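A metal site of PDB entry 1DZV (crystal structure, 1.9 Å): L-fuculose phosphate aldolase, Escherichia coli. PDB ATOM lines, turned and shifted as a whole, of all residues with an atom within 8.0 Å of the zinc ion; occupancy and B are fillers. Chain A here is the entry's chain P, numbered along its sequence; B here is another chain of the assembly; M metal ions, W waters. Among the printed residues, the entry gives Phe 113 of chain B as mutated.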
ATOM      1  N   THR A  26      12.384  -8.103 -18.141  1.00  0.00           N
ATOM      2  CA  THR A  26      13.665  -8.624 -17.677  1.00  0.00           C
ATOM      3  C   THR A  26      14.367  -9.484 -18.711  1.00  0.00           C
ATOM      4  O   THR A  26      15.353 -10.166 -18.402  1.00  0.00           O
ATOM      5  CB  THR A  26      13.368  -9.475 -16.407  1.00  0.00           C
ATOM      6  OG1 THR A  26      12.379 -10.466 -16.732  1.00  0.00           O
ATOM      7  CG2 THR A  26      12.866  -8.581 -15.284  1.00  0.00           C
ATOM      8  N   ALA A  27      13.906  -9.450 -19.953  1.00  0.00           N
ATOM      9  CA  ALA A  27      14.393 -10.306 -21.013  1.00  0.00           C
ATOM     10  C   ALA A  27      15.852 -10.216 -21.405  1.00  0.00           C
ATOM     11  O   ALA A  27      16.445 -11.282 -21.649  1.00  0.00           O
ATOM     12  CB  ALA A  27      13.479 -10.115 -22.223  1.00  0.00           C
ATOM     13  N   GLY A  28      16.526  -9.090 -21.531  1.00  0.00           N
ATOM     14  CA  GLY A  28      17.908  -9.135 -22.020  1.00  0.00           C
ATOM     15  C   GLY A  28      18.986  -9.554 -21.035  1.00  0.00           C
ATOM     16  O   GLY A  28      18.792  -9.640 -19.824  1.00  0.00           O
ATOM     17  N   ASN A  29      20.171  -9.886 -21.578  1.00  0.00           N
ATOM     18  CA  ASN A  29      21.357 -10.191 -20.786  1.00  0.00           C
ATOM     19  C   ASN A  29      22.546  -9.714 -21.634  1.00  0.00           C
ATOM     20  O   ASN A  29      22.516  -9.688 -22.868  1.00  0.00           O
ATOM     21  CB  ASN A  29      21.516 -11.615 -20.301  1.00  0.00           C
ATOM     22  CG  ASN A  29      20.861 -12.663 -21.161  1.00  0.00           C
ATOM     23  OD1 ASN A  29      21.431 -13.047 -22.181  1.00  0.00           O
ATOM     24  ND2 ASN A  29      19.662 -13.107 -20.775  1.00  0.00           N
ATOM     25  N   SER A  71      22.960 -14.735 -15.157  1.00  0.00           N
ATOM     26  CA  SER A  71      21.837 -14.839 -16.069  1.00  0.00           C
ATOM     27  C   SER A  71      21.588 -16.319 -16.323  1.00  0.00           C
ATOM     28  O   SER A  71      22.568 -17.055 -16.531  1.00  0.00           O
ATOM     29  CB  SER A  71      22.245 -14.193 -17.410  1.00  0.00           C
ATOM     30  OG  SER A  71      21.333 -14.589 -18.417  1.00  0.00           O
ATOM     31  N   SER A  72      20.325 -16.692 -16.505  1.00  0.00           N
ATOM     32  CA  SER A  72      20.075 -18.118 -16.762  1.00  0.00           C
ATOM     33  C   SER A  72      20.518 -18.519 -18.161  1.00  0.00           C
ATOM     34  O   SER A  72      20.596 -19.727 -18.421  1.00  0.00           O
ATOM     35  CB  SER A  72      18.608 -18.470 -16.525  1.00  0.00           C
ATOM     36  OG  SER A  72      17.869 -17.948 -17.621  1.00  0.00           O
ATOM     37  N   GLU A  73      20.886 -17.581 -19.024  1.00  0.00           N
ATOM     38  CA  GLU A  73      21.350 -17.869 -20.361  1.00  0.00           C
ATOM     39  C   GLU A  73      22.841 -17.669 -20.535  1.00  0.00           C
ATOM     40  O   GLU A  73      23.331 -17.549 -21.669  1.00  0.00           O
ATOM     41  CB  GLU A  73      20.581 -16.952 -21.343  1.00  0.00           C
ATOM     42  CG  GLU A  73      19.073 -17.082 -21.091  1.00  0.00           C
ATOM     43  CD  GLU A  73      18.227 -16.383 -22.125  1.00  0.00           C
ATOM     44  OE1 GLU A  73      17.883 -17.028 -23.132  1.00  0.00           O
ATOM     45  OE2 GLU A  73      17.928 -15.186 -21.918  1.00  0.00           O
ATOM     46  N   PHE A  76      25.174 -19.660 -23.490  1.00  0.00           N
ATOM     47  CA  PHE A  76      25.400 -19.264 -24.896  1.00  0.00           C
ATOM     48  C   PHE A  76      26.260 -18.006 -24.940  1.00  0.00           C
ATOM     49  O   PHE A  76      26.824 -17.779 -26.009  1.00  0.00           O
ATOM     50  CB  PHE A  76      24.163 -19.278 -25.738  1.00  0.00           C
ATOM     51  CG  PHE A  76      23.047 -18.333 -25.464  1.00  0.00           C
ATOM     52  CD1 PHE A  76      23.267 -16.999 -25.151  1.00  0.00           C
ATOM     53  CD2 PHE A  76      21.729 -18.793 -25.551  1.00  0.00           C
ATOM     54  CE1 PHE A  76      22.182 -16.150 -24.911  1.00  0.00           C
ATOM     55  CE2 PHE A  76      20.655 -17.934 -25.311  1.00  0.00           C
ATOM     56  CZ  PHE A  76      20.905 -16.612 -24.990  1.00  0.00           C
ATOM     57  N   HIS A  77      26.471 -17.249 -23.871  1.00  0.00           N
ATOM     58  CA  HIS A  77      27.454 -16.157 -23.911  1.00  0.00           C
ATOM     59  C   HIS A  77      28.843 -16.793 -23.990  1.00  0.00           C
ATOM     60  O   HIS A  77      29.701 -16.447 -24.822  1.00  0.00           O
ATOM     61  CB  HIS A  77      27.346 -15.273 -22.655  1.00  0.00           C
ATOM     62  CG  HIS A  77      26.145 -14.381 -22.694  1.00  0.00           C
ATOM     63  ND1 HIS A  77      26.283 -13.010 -22.879  1.00  0.00           N
ATOM     64  CD2 HIS A  77      24.830 -14.647 -22.606  1.00  0.00           C
ATOM     65  CE1 HIS A  77      25.060 -12.468 -22.897  1.00  0.00           C
ATOM     66  NE2 HIS A  77      24.153 -13.436 -22.750  1.00  0.00           N
ATOM     67  N   HIS A  92      22.165  -9.903 -25.791  1.00  0.00           N
ATOM     68  CA  HIS A  92      21.068 -10.818 -26.136  1.00  0.00           C
ATOM     69  C   HIS A  92      19.759 -10.134 -25.781  1.00  0.00           C
ATOM     70  O   HIS A  92      19.653  -9.576 -24.687  1.00  0.00           O
ATOM     71  CB  HIS A  92      21.217 -12.158 -25.398  1.00  0.00           C
ATOM     72  CG  HIS A  92      19.988 -13.016 -25.487  1.00  0.00           C
ATOM     73  ND1 HIS A  92      19.435 -13.445 -26.684  1.00  0.00           N
ATOM     74  CD2 HIS A  92      19.183 -13.483 -24.504  1.00  0.00           C
ATOM     75  CE1 HIS A  92      18.356 -14.175 -26.418  1.00  0.00           C
ATOM     76  NE2 HIS A  92      18.187 -14.185 -25.099  1.00  0.00           N
ATOM     77  N   ASN A  93      18.744 -10.200 -26.630  1.00  0.00           N
ATOM     78  CA  ASN A  93      17.470  -9.616 -26.175  1.00  0.00           C
ATOM     79  C   ASN A  93      16.381 -10.362 -26.925  1.00  0.00           C
ATOM     80  O   ASN A  93      16.659 -11.243 -27.756  1.00  0.00           O
ATOM     81  CB  ASN A  93      17.463  -8.118 -26.419  1.00  0.00           C
ATOM     82  CG  ASN A  93      17.637  -7.750 -27.888  1.00  0.00           C
ATOM     83  OD1 ASN A  93      16.986  -8.334 -28.758  1.00  0.00           O
ATOM     84  ND2 ASN A  93      18.504  -6.760 -28.178  1.00  0.00           N
ATOM     85  N   HIS A  94      15.147 -10.040 -26.595  1.00  0.00           N
ATOM     86  CA  HIS A  94      13.968 -10.575 -27.235  1.00  0.00           C
ATOM     87  C   HIS A  94      13.258  -9.430 -27.973  1.00  0.00           C
ATOM     88  O   HIS A  94      12.063  -9.232 -27.845  1.00  0.00           O
ATOM     89  CB  HIS A  94      13.048 -11.291 -26.254  1.00  0.00           C
ATOM     90  CG  HIS A  94      13.615 -12.387 -25.406  1.00  0.00           C
ATOM     91  ND1 HIS A  94      12.883 -12.994 -24.411  1.00  0.00           N
ATOM     92  CD2 HIS A  94      14.818 -13.010 -25.405  1.00  0.00           C
ATOM     93  CE1 HIS A  94      13.628 -13.916 -23.806  1.00  0.00           C
ATOM     94  NE2 HIS A  94      14.825 -13.948 -24.406  1.00  0.00           N
ATOM     95  N   PHE A 131      15.938 -22.870 -23.507  1.00  0.00           N
ATOM     96  CA  PHE A 131      16.918 -21.900 -23.026  1.00  0.00           C
ATOM     97  C   PHE A 131      17.798 -22.553 -21.951  1.00  0.00           C
ATOM     98  O   PHE A 131      17.374 -23.430 -21.198  1.00  0.00           O
ATOM     99  CB  PHE A 131      16.285 -20.634 -22.440  1.00  0.00           C
ATOM    100  CG  PHE A 131      15.580 -20.845 -21.130  1.00  0.00           C
ATOM    101  CD1 PHE A 131      14.306 -21.374 -21.093  1.00  0.00           C
ATOM    102  CD2 PHE A 131      16.202 -20.533 -19.926  1.00  0.00           C
ATOM    103  CE1 PHE A 131      13.647 -21.582 -19.885  1.00  0.00           C
ATOM    104  CE2 PHE A 131      15.556 -20.744 -18.723  1.00  0.00           C
ATOM    105  CZ  PHE A 131      14.276 -21.266 -18.689  1.00  0.00           C
ATOM    106  N   GLY A 132      19.057 -22.113 -21.885  1.00  0.00           N
ATOM    107  CA  GLY A 132      20.004 -22.567 -20.895  1.00  0.00           C
ATOM    108  C   GLY A 132      20.640 -23.920 -21.112  1.00  0.00           C
ATOM    109  O   GLY A 132      21.361 -24.390 -20.212  1.00  0.00           O
ATOM    110  N   LEU A 136      21.290 -25.716 -27.091  1.00  0.00           N
ATOM    111  CA  LEU A 136      21.118 -24.352 -27.589  1.00  0.00           C
ATOM    112  C   LEU A 136      22.480 -23.698 -27.890  1.00  0.00           C
ATOM    113  O   LEU A 136      22.673 -23.122 -28.957  1.00  0.00           O
ATOM    114  CB  LEU A 136      20.413 -23.458 -26.570  1.00  0.00           C
ATOM    115  CG  LEU A 136      19.410 -22.404 -27.014  1.00  0.00           C
ATOM    116  CD1 LEU A 136      19.298 -21.223 -26.051  1.00  0.00           C
ATOM    117  CD2 LEU A 136      19.603 -21.961 -28.442  1.00  0.00           C
ATOM    118  N   LEU A 152      17.364 -16.578 -33.028  1.00  0.00           N
ATOM    119  CA  LEU A 152      17.218 -17.881 -32.331  1.00  0.00           C
ATOM    120  C   LEU A 152      15.734 -18.255 -32.458  1.00  0.00           C
ATOM    121  O   LEU A 152      14.915 -17.506 -31.930  1.00  0.00           O
ATOM    122  CB  LEU A 152      17.565 -17.709 -30.857  1.00  0.00           C
ATOM    123  CG  LEU A 152      19.057 -17.512 -30.502  1.00  0.00           C
ATOM    124  CD1 LEU A 152      19.467 -16.069 -30.717  1.00  0.00           C
ATOM    125  CD2 LEU A 152      19.276 -17.826 -29.030  1.00  0.00           C
ATOM    126  N   HIS A 154      11.986 -19.108 -32.186  1.00  0.00           N
ATOM    127  CA  HIS A 154      11.039 -18.963 -31.101  1.00  0.00           C
ATOM    128  C   HIS A 154      11.659 -18.315 -29.861  1.00  0.00           C
ATOM    129  O   HIS A 154      11.288 -18.648 -28.722  1.00  0.00           O
ATOM    130  CB  HIS A 154      10.414 -20.309 -30.659  1.00  0.00           C
ATOM    131  CG  HIS A 154       9.472 -20.881 -31.651  1.00  0.00           C
ATOM    132  ND1 HIS A 154       8.206 -20.365 -31.899  1.00  0.00           N
ATOM    133  CD2 HIS A 154       9.619 -21.954 -32.482  1.00  0.00           C
ATOM    134  CE1 HIS A 154       7.631 -21.105 -32.849  1.00  0.00           C
ATOM    135  NE2 HIS A 154       8.464 -22.067 -33.223  1.00  0.00           N
ATOM    136  N   HIS A 155      12.573 -17.346 -30.058  1.00  0.00           N
ATOM    137  CA  HIS A 155      13.246 -16.858 -28.851  1.00  0.00           C
ATOM    138  C   HIS A 155      13.687 -15.409 -28.973  1.00  0.00           C
ATOM    139  O   HIS A 155      13.170 -14.571 -28.230  1.00  0.00           O
ATOM    140  CB  HIS A 155      14.436 -17.813 -28.647  1.00  0.00           C
ATOM    141  CG  HIS A 155      15.202 -17.562 -27.398  1.00  0.00           C
ATOM    142  ND1 HIS A 155      15.856 -18.583 -26.753  1.00  0.00           N
ATOM    143  CD2 HIS A 155      15.423 -16.450 -26.653  1.00  0.00           C
ATOM    144  CE1 HIS A 155      16.445 -18.089 -25.665  1.00  0.00           C
ATOM    145  NE2 HIS A 155      16.215 -16.789 -25.575  1.00  0.00           N
ATOM    146  N   GLY A 156      14.651 -15.125 -29.854  1.00  0.00           N
ATOM    147  CA  GLY A 156      15.138 -13.735 -29.905  1.00  0.00           C
ATOM    148  C   GLY A 156      16.408 -13.575 -30.705  1.00  0.00           C
ATOM    149  O   GLY A 156      16.566 -14.211 -31.759  1.00  0.00           O
ATOM    150  N   LEU A 157      17.328 -12.739 -30.245  1.00  0.00           N
ATOM    151  CA  LEU A 157      18.517 -12.335 -30.983  1.00  0.00           C
ATOM    152  C   LEU A 157      19.801 -12.392 -30.148  1.00  0.00           C
ATOM    153  O   LEU A 157      19.765 -12.025 -28.982  1.00  0.00           O
ATOM    154  CB  LEU A 157      18.318 -10.869 -31.367  1.00  0.00           C
ATOM    155  CG  LEU A 157      19.309  -9.907 -32.010  1.00  0.00           C
ATOM    156  CD1 LEU A 157      20.382  -9.446 -31.038  1.00  0.00           C
ATOM    157  CD2 LEU A 157      19.966 -10.415 -33.276  1.00  0.00           C
ATOM    158  N   ILE A 158      20.939 -12.704 -30.785  1.00  0.00           N
ATOM    159  CA  ILE A 158      22.244 -12.596 -30.169  1.00  0.00           C
ATOM    160  C   ILE A 158      23.131 -11.813 -31.147  1.00  0.00           C
ATOM    161  O   ILE A 158      23.141 -12.091 -32.351  1.00  0.00           O
ATOM    162  CB  ILE A 158      22.914 -13.936 -29.818  1.00  0.00           C
ATOM    163  CG1 ILE A 158      22.558 -14.348 -28.396  1.00  0.00           C
ATOM    164  CG2 ILE A 158      24.425 -13.882 -30.017  1.00  0.00           C
ATOM    165  CD1 ILE A 158      23.714 -14.673 -27.466  1.00  0.00           C
ATOM    166  N   HIS B 112       6.000 -18.565 -28.479  1.00  0.00           N
ATOM    167  CA  HIS B 112       7.234 -18.194 -27.811  1.00  0.00           C
ATOM    168  C   HIS B 112       7.235 -18.845 -26.438  1.00  0.00           C
ATOM    169  O   HIS B 112       6.133 -18.990 -25.866  1.00  0.00           O
ATOM    170  CB  HIS B 112       7.285 -16.667 -27.619  1.00  0.00           C
ATOM    171  CG  HIS B 112       8.652 -16.157 -27.253  1.00  0.00           C
ATOM    172  ND1 HIS B 112       9.152 -16.244 -25.986  1.00  0.00           N
ATOM    173  CD2 HIS B 112       9.624 -15.613 -28.023  1.00  0.00           C
ATOM    174  CE1 HIS B 112      10.372 -15.751 -25.945  1.00  0.00           C
ATOM    175  NE2 HIS B 112      10.691 -15.342 -27.168  1.00  0.00           N
ATOM    176  N   PHE B 113       8.392 -19.213 -25.895  1.00  0.00           N
ATOM    177  CA  PHE B 113       8.383 -19.905 -24.611  1.00  0.00           C
ATOM    178  C   PHE B 113       7.999 -19.036 -23.432  1.00  0.00           C
ATOM    179  O   PHE B 113       7.533 -19.588 -22.420  1.00  0.00           O
ATOM    180  CB  PHE B 113       9.704 -20.637 -24.361  1.00  0.00           C
ATOM    181  CG  PHE B 113      10.834 -19.672 -24.151  1.00  0.00           C
ATOM    182  CD1 PHE B 113      11.130 -19.205 -22.899  1.00  0.00           C
ATOM    183  CD2 PHE B 113      11.590 -19.277 -25.246  1.00  0.00           C
ATOM    184  CE1 PHE B 113      12.179 -18.309 -22.713  1.00  0.00           C
ATOM    185  CE2 PHE B 113      12.647 -18.390 -25.071  1.00  0.00           C
ATOM    186  CZ  PHE B 113      12.928 -17.918 -23.801  1.00  0.00           C
ATOM    187  N   MET B 114       8.017 -17.712 -23.520  1.00  0.00           N
ATOM    188  CA  MET B 114       7.570 -16.890 -22.424  1.00  0.00           C
ATOM    189  C   MET B 114       6.067 -16.973 -22.173  1.00  0.00           C
ATOM    190  O   MET B 114       5.619 -16.482 -21.130  1.00  0.00           O
ATOM    191  CB  MET B 114       7.982 -15.428 -22.628  1.00  0.00           C
ATOM    192  CG  MET B 114       9.477 -15.255 -22.385  1.00  0.00           C
ATOM    193  SD  MET B 114       9.945 -15.589 -20.673  1.00  0.00           S
ATOM    194  CE  MET B 114       8.873 -14.444 -19.815  1.00  0.00           C
HETATM  195 ZN    ZN M   1      16.612 -15.214 -24.134  1.00  0.00          ZN
HETATM  196  O   HOH W   1      16.201 -13.686 -21.017  1.00  0.00           O
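The backbone carbonyl oxygen of Asn 29 lies within hydrogen-bond range of the backbone NH of His 92, 3.0 Å away. The backbone carbonyl oxygen of Leu 157 lies within hydrogen-bond range of a ring nitrogen (ND1) of His 92 (2.7 Å). The backbone carbonyl oxygen (O) of His 155 is in hydrogen-bond range of a ring nitrogen (NE2) of His 112 of chain B, 2.8 Å away. The side-chain carboxylate of Glu 73 lies close to the side-chain amide nitrogen of Asn 29 (2.9 Å). The side-chain hydroxyl (OG) of Ser 71 sits close to the backbone NH (N) of Glu 73 (3.1 Å).
Within 4 Å of the zinc ion: Glu 73, His 92, His 94 and His 155.
The zinc ion is bound by a ring nitrogen (NE2) of His 92 (2.1 Å), a ring nitrogen (NE2) of His 155 (2.2 Å), a ring nitrogen (NE2) of His 94 (2.2 Å), the side-chain carboxylate (OE1) of Glu 73 (2.4 Å) and the side-chain carboxylate (OE2) of Glu 73 (2.6 Å).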
